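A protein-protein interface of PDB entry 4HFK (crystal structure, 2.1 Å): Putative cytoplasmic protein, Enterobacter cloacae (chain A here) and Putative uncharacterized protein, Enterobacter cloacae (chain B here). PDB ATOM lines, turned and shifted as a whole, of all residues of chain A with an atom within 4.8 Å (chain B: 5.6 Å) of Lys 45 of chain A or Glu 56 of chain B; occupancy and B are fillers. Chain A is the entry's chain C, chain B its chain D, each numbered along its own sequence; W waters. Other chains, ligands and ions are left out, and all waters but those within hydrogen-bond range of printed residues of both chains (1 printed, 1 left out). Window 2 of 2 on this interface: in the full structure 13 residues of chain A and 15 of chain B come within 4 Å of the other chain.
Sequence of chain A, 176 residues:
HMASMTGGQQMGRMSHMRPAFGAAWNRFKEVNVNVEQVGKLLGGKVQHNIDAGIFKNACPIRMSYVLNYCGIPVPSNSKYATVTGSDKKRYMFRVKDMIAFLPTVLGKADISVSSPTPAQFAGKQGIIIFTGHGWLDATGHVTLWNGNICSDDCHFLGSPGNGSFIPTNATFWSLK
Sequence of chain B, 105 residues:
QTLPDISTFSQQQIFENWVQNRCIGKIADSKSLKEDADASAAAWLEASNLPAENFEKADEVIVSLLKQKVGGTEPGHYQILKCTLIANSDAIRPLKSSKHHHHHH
Of the 11 printed residues of chain A, 4 touch a printed residue of chain B.
Hydrophobic or aromatic side chains of chain A that line the printed part of chain B: Ile 54 and Val 83.
Along chain A the printed residues that touch a printed residue of chain B span positions 45 to 83.
Among the printed residues, 5 pairs touch across the chains.
Among the printed residues, Asp or Glu carboxylates within 4 Å of a Lys or Arg side-chain nitrogen of the other chain: Lys 45 of chain A with Glu 56 of chain B (3.0 Å).
Water W1 bridges the backbone carbonyl oxygen (O) of Ile 54 of chain A (2.7 Å) and the indole nitrogen (NE1) of Trp 18 of chain B (2.9 Å).
NZ of Lys 45 of chain A lies within salt-bridge range of OE1 of Glu 56 of chain B (3.0 Å).
The side-chain amide nitrogen of Asn 49 of chain A is in hydrogen-bond range of the side-chain carboxylate of Glu 56 of chain B (2.9 Å).
The backbone NH (N) of Lys 45 of chain A lies within hydrogen-bond range of the backbone carbonyl oxygen (O) of Thr 84 of chain A.
ND1 of His 48 of chain A lies within hydrogen-bond range of OD1 of Asn 49 of chain A (3.3 Å).
O of Asn 49 of chain A sits at hydrogen-bond distance from N of Ile 54 of chain A (3.0 Å).
Ile 54 of chain A touches Trp 18 of chain B.
CG1 of Val 83 of chain A touches CB of Ala 52 of chain B, 3.4 Å away.
OE2 of Glu 56 of chain B touches CG1 of Val 83 of chain A, at 3.99 Å.
Lys 45 of chain A touches one residue of chain B.
Printed residues of chain B within 4 Å of Asn 49 of chain A: Glu 56.
Of the printed residues of chain B, Ile 54 of chain A touches Trp 18 (3.99 Å).
Of the printed residues of chain B, Val 83 of chain A touches Ala 52 and Glu 56.
Printed residues of chain A within 4 Å of Trp 18 of chain B: Ile 54 (3.99 Å).
Printed residues of chain A within 4 Å of Ala 52 of chain B: Val 83.
Of the printed residues of chain A, Glu 56 of chain B touches Lys 45 (3.0 Å), Asn 49 (2.9 Å) and Val 83 (3.99 Å).
Ala 58 of chain B touches none of the printed residues of chain A.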
ATOM      1  N   GLY A  43      20.100   1.212  14.540  1.00  0.00           N
ATOM      2  CA  GLY A  43      20.525   2.533  14.988  1.00  0.00           C
ATOM      3  C   GLY A  43      20.413   3.581  13.890  1.00  0.00           C
ATOM      4  O   GLY A  43      19.759   3.356  12.862  1.00  0.00           O
ATOM      5  N   GLY A  44      21.040   4.733  14.113  1.00  0.00           N
ATOM      6  CA  GLY A  44      21.155   5.770  13.102  1.00  0.00           C
ATOM      7  C   GLY A  44      19.845   6.419  12.675  1.00  0.00           C
ATOM      8  O   GLY A  44      18.926   6.580  13.478  1.00  0.00           O
ATOM      9  N   LYS A  45      19.765   6.792  11.404  1.00  0.00           N
ATOM     10  CA  LYS A  45      18.556   7.397  10.850  1.00  0.00           C
ATOM     11  C   LYS A  45      17.388   6.408  10.836  1.00  0.00           C
ATOM     12  O   LYS A  45      16.229   6.790  11.066  1.00  0.00           O
ATOM     13  CB  LYS A  45      18.821   7.881   9.427  1.00  0.00           C
ATOM     14  CG  LYS A  45      18.734   9.364   9.254  1.00  0.00           C
ATOM     15  CD  LYS A  45      17.447   9.912   9.828  1.00  0.00           C
ATOM     16  CE  LYS A  45      17.764  11.186  10.579  1.00  0.00           C
ATOM     17  NZ  LYS A  45      18.560  12.103   9.722  1.00  0.00           N
ATOM     18  N   VAL A  46      17.687   5.142  10.548  1.00  0.00           N
ATOM     19  CA  VAL A  46      16.671   4.091  10.596  1.00  0.00           C
ATOM     20  C   VAL A  46      15.948   4.093  11.937  1.00  0.00           C
ATOM     21  O   VAL A  46      14.712   4.151  11.989  1.00  0.00           O
ATOM     22  CB  VAL A  46      17.284   2.696  10.371  1.00  0.00           C
ATOM     23  CG1 VAL A  46      16.262   1.615  10.698  1.00  0.00           C
ATOM     24  CG2 VAL A  46      17.772   2.553   8.941  1.00  0.00           C
ATOM     25  N   GLN A  47      16.718   4.042  13.022  1.00  0.00           N
ATOM     26  CA  GLN A  47      16.143   4.050  14.368  1.00  0.00           C
ATOM     27  C   GLN A  47      15.377   5.338  14.679  1.00  0.00           C
ATOM     28  O   GLN A  47      14.305   5.301  15.293  1.00  0.00           O
ATOM     29  CB  GLN A  47      17.218   3.828  15.450  1.00  0.00           C
ATOM     30  CG  GLN A  47      16.631   3.862  16.875  1.00  0.00           C
ATOM     31  CD  GLN A  47      17.638   3.510  17.968  1.00  0.00           C
ATOM     32  OE1 GLN A  47      18.814   3.302  17.690  1.00  0.00           O
ATOM     33  NE2 GLN A  47      17.174   3.455  19.222  1.00  0.00           N
ATOM     34  N   HIS A  48      15.940   6.472  14.276  1.00  0.00           N
ATOM     35  CA  HIS A  48      15.311   7.765  14.521  1.00  0.00           C
ATOM     36  C   HIS A  48      13.905   7.800  13.931  1.00  0.00           C
ATOM     37  O   HIS A  48      12.945   8.171  14.614  1.00  0.00           O
ATOM     38  CB  HIS A  48      16.150   8.898  13.926  1.00  0.00           C
ATOM     39  CG  HIS A  48      15.563  10.254  14.151  1.00  0.00           C
ATOM     40  ND1 HIS A  48      14.715  10.859  13.250  1.00  0.00           N
ATOM     41  CD2 HIS A  48      15.692  11.117  15.189  1.00  0.00           C
ATOM     42  CE1 HIS A  48      14.349  12.040  13.719  1.00  0.00           C
ATOM     43  NE2 HIS A  48      14.927  12.217  14.894  1.00  0.00           N
ATOM     44  N   ASN A  49      13.780   7.396  12.669  1.00  0.00           N
ATOM     45  CA  ASN A  49      12.486   7.449  11.989  1.00  0.00           C
ATOM     46  C   ASN A  49      11.499   6.396  12.500  1.00  0.00           C
ATOM     47  O   ASN A  49      10.291   6.633  12.518  1.00  0.00           O
ATOM     48  CB  ASN A  49      12.656   7.381  10.467  1.00  0.00           C
ATOM     49  CG  ASN A  49      13.301   8.633   9.916  1.00  0.00           C
ATOM     50  OD1 ASN A  49      13.264   9.677  10.563  1.00  0.00           O
ATOM     51  ND2 ASN A  49      13.900   8.540   8.732  1.00  0.00           N
ATOM     52  N   ILE A  54       7.402   7.298  12.245  1.00  0.00           N
ATOM     53  CA  ILE A  54       7.278   7.559  10.809  1.00  0.00           C
ATOM     54  C   ILE A  54       7.429   6.280   9.955  1.00  0.00           C
ATOM     55  O   ILE A  54       6.661   6.056   8.998  1.00  0.00           O
ATOM     56  CB  ILE A  54       8.300   8.639  10.361  1.00  0.00           C
ATOM     57  CG1 ILE A  54       7.986   9.999  11.009  1.00  0.00           C
ATOM     58  CG2 ILE A  54       8.328   8.762   8.835  1.00  0.00           C
ATOM     59  CD1 ILE A  54       9.129  11.029  10.865  1.00  0.00           C
ATOM     60  N   VAL A  83      17.542   5.482   3.925  1.00  0.00           N
ATOM     61  CA  VAL A  83      18.217   6.185   5.022  1.00  0.00           C
ATOM     62  C   VAL A  83      19.348   5.294   5.537  1.00  0.00           C
ATOM     63  O   VAL A  83      19.373   4.099   5.258  1.00  0.00           O
ATOM     64  CB  VAL A  83      17.272   6.532   6.206  1.00  0.00           C
ATOM     65  CG1 VAL A  83      16.181   7.497   5.763  1.00  0.00           C
ATOM     66  CG2 VAL A  83      16.667   5.274   6.806  1.00  0.00           C
ATOM     67  N   THR A  84      20.273   5.864   6.300  1.00  0.00           N
ATOM     68  CA  THR A  84      21.404   5.087   6.794  1.00  0.00           C
ATOM     69  C   THR A  84      21.148   4.527   8.179  1.00  0.00           C
ATOM     70  O   THR A  84      20.442   5.138   8.984  1.00  0.00           O
ATOM     71  CB  THR A  84      22.673   5.936   6.834  1.00  0.00           C
ATOM     72  OG1 THR A  84      22.427   7.112   7.618  1.00  0.00           O
ATOM     73  CG2 THR A  84      23.069   6.350   5.422  1.00  0.00           C
ATOM     74  N   GLY A  85      21.717   3.356   8.457  1.00  0.00           N
ATOM     75  CA  GLY A  85      21.732   2.843   9.814  1.00  0.00           C
ATOM     76  C   GLY A  85      22.996   3.349  10.495  1.00  0.00           C
ATOM     77  O   GLY A  85      23.785   4.074   9.880  1.00  0.00           O
ATOM     78  N   TRP B  18      -0.335  12.941   4.496  1.00  0.00           N
ATOM     79  CA  TRP B  18       0.592  12.383   5.473  1.00  0.00           C
ATOM     80  C   TRP B  18       0.714  13.361   6.637  1.00  0.00           C
ATOM     81  O   TRP B  18       0.584  12.980   7.801  1.00  0.00           O
ATOM     82  CB  TRP B  18       1.974  12.145   4.853  1.00  0.00           C
ATOM     83  CG  TRP B  18       2.969  11.584   5.850  1.00  0.00           C
ATOM     84  CD1 TRP B  18       3.184  10.264   6.137  1.00  0.00           C
ATOM     85  CD2 TRP B  18       3.860  12.329   6.695  1.00  0.00           C
ATOM     86  NE1 TRP B  18       4.151  10.141   7.105  1.00  0.00           N
ATOM     87  CE2 TRP B  18       4.584  11.393   7.463  1.00  0.00           C
ATOM     88  CE3 TRP B  18       4.120  13.695   6.873  1.00  0.00           C
ATOM     89  CZ2 TRP B  18       5.557  11.782   8.389  1.00  0.00           C
ATOM     90  CZ3 TRP B  18       5.085  14.080   7.802  1.00  0.00           C
ATOM     91  CH2 TRP B  18       5.791  13.126   8.543  1.00  0.00           C
ATOM     92  N   ALA B  52      13.045  10.492   2.542  1.00  0.00           N
ATOM     93  CA  ALA B  52      12.689  10.410   3.957  1.00  0.00           C
ATOM     94  C   ALA B  52      12.893  11.738   4.675  1.00  0.00           C
ATOM     95  O   ALA B  52      12.121  12.108   5.566  1.00  0.00           O
ATOM     96  CB  ALA B  52      13.509   9.335   4.632  1.00  0.00           C
ATOM     97  N   GLU B  53      13.947  12.443   4.281  1.00  0.00           N
ATOM     98  CA  GLU B  53      14.320  13.703   4.904  1.00  0.00           C
ATOM     99  C   GLU B  53      13.163  14.703   4.896  1.00  0.00           C
ATOM    100  O   GLU B  53      12.993  15.476   5.844  1.00  0.00           O
ATOM    101  CB  GLU B  53      15.540  14.298   4.186  1.00  0.00           C
ATOM    102  CG  GLU B  53      16.050  15.575   4.811  1.00  0.00           C
ATOM    103  CD  GLU B  53      17.404  15.996   4.271  1.00  0.00           C
ATOM    104  OE1 GLU B  53      17.521  16.179   3.041  1.00  0.00           O
ATOM    105  OE2 GLU B  53      18.346  16.140   5.083  1.00  0.00           O
ATOM    106  N   ASN B  54      12.364  14.693   3.833  1.00  0.00           N
ATOM    107  CA  ASN B  54      11.216  15.597   3.771  1.00  0.00           C
ATOM    108  C   ASN B  54      10.238  15.320   4.908  1.00  0.00           C
ATOM    109  O   ASN B  54       9.681  16.241   5.505  1.00  0.00           O
ATOM    110  CB  ASN B  54      10.510  15.500   2.412  1.00  0.00           C
ATOM    111  CG  ASN B  54      11.395  15.954   1.276  1.00  0.00           C
ATOM    112  OD1 ASN B  54      12.536  15.498   1.145  1.00  0.00           O
ATOM    113  ND2 ASN B  54      10.887  16.870   0.457  1.00  0.00           N
ATOM    114  N   PHE B  55      10.049  14.042   5.213  1.00  0.00           N
ATOM    115  CA  PHE B  55       9.147  13.639   6.286  1.00  0.00           C
ATOM    116  C   PHE B  55       9.735  13.916   7.676  1.00  0.00           C
ATOM    117  O   PHE B  55       9.024  14.387   8.583  1.00  0.00           O
ATOM    118  CB  PHE B  55       8.766  12.163   6.105  1.00  0.00           C
ATOM    119  CG  PHE B  55       8.036  11.891   4.810  1.00  0.00           C
ATOM    120  CD1 PHE B  55       6.648  11.996   4.746  1.00  0.00           C
ATOM    121  CD2 PHE B  55       8.733  11.554   3.655  1.00  0.00           C
ATOM    122  CE1 PHE B  55       5.965  11.758   3.554  1.00  0.00           C
ATOM    123  CE2 PHE B  55       8.052  11.321   2.451  1.00  0.00           C
ATOM    124  CZ  PHE B  55       6.670  11.424   2.405  1.00  0.00           C
ATOM    125  N   GLU B  56      11.028  13.634   7.844  1.00  0.00           N
ATOM    126  CA  GLU B  56      11.719  13.931   9.098  1.00  0.00           C
ATOM    127  C   GLU B  56      11.588  15.416   9.447  1.00  0.00           C
ATOM    128  O   GLU B  56      11.272  15.778  10.581  1.00  0.00           O
ATOM    129  CB  GLU B  56      13.213  13.593   8.985  1.00  0.00           C
ATOM    130  CG  GLU B  56      13.519  12.143   8.677  1.00  0.00           C
ATOM    131  CD  GLU B  56      14.980  11.927   8.298  1.00  0.00           C
ATOM    132  OE1 GLU B  56      15.827  12.797   8.640  1.00  0.00           O
ATOM    133  OE2 GLU B  56      15.269  10.894   7.640  1.00  0.00           O
ATOM    134  N   LYS B  57      11.852  16.281   8.473  1.00  0.00           N
ATOM    135  CA  LYS B  57      11.783  17.724   8.711  1.00  0.00           C
ATOM    136  C   LYS B  57      10.346  18.183   8.915  1.00  0.00           C
ATOM    137  O   LYS B  57      10.067  19.026   9.771  1.00  0.00           O
ATOM    138  CB  LYS B  57      12.424  18.487   7.550  1.00  0.00           C
ATOM    139  CG  LYS B  57      13.954  18.374   7.509  1.00  0.00           C
ATOM    140  CD  LYS B  57      14.500  18.940   6.199  1.00  0.00           C
ATOM    141  CE  LYS B  57      16.023  18.934   6.162  1.00  0.00           C
ATOM    142  NZ  LYS B  57      16.515  19.273   4.793  1.00  0.00           N
ATOM    143  N   ALA B  58       9.428  17.617   8.137  1.00  0.00           N
ATOM    144  CA  ALA B  58       8.017  17.978   8.271  1.00  0.00           C
ATOM    145  C   ALA B  58       7.487  17.671   9.677  1.00  0.00           C
ATOM    146  O   ALA B  58       6.720  18.453  10.251  1.00  0.00           O
ATOM    147  CB  ALA B  58       7.187  17.281   7.207  1.00  0.00           C
ATOM    148  N   ASP B  59       7.909  16.542  10.238  1.00  0.00           N
ATOM    149  CA  ASP B  59       7.444  16.149  11.564  1.00  0.00           C
ATOM    150  C   ASP B  59       7.889  17.186  12.605  1.00  0.00           C
ATOM    151  O   ASP B  59       7.154  17.481  13.547  1.00  0.00           O
ATOM    152  CB  ASP B  59       7.941  14.739  11.919  1.00  0.00           C
ATOM    153  CG  ASP B  59       7.001  14.002  12.869  1.00  0.00           C
ATOM    154  OD1 ASP B  59       5.856  13.679  12.467  1.00  0.00           O
ATOM    155  OD2 ASP B  59       7.409  13.712  14.011  1.00  0.00           O
ATOM    156  N   GLU B  60       9.071  17.765  12.422  1.00  0.00           N
ATOM    157  CA  GLU B  60       9.523  18.830  13.324  1.00  0.00           C
ATOM    158  C   GLU B  60       8.708  20.108  13.124  1.00  0.00           C
ATOM    159  O   GLU B  60       8.388  20.809  14.087  1.00  0.00           O
ATOM    160  CB  GLU B  60      11.011  19.112  13.119  1.00  0.00           C
ATOM    161  CG  GLU B  60      11.902  17.907  13.429  1.00  0.00           C
ATOM    162  CD  GLU B  60      13.337  18.095  12.949  1.00  0.00           C
ATOM    163  OE1 GLU B  60      13.673  19.205  12.479  1.00  0.00           O
ATOM    164  OE2 GLU B  60      14.123  17.127  13.043  1.00  0.00           O
HETATM  165  O   HOH W   1       4.519   7.604   8.363  1.00  0.00           O
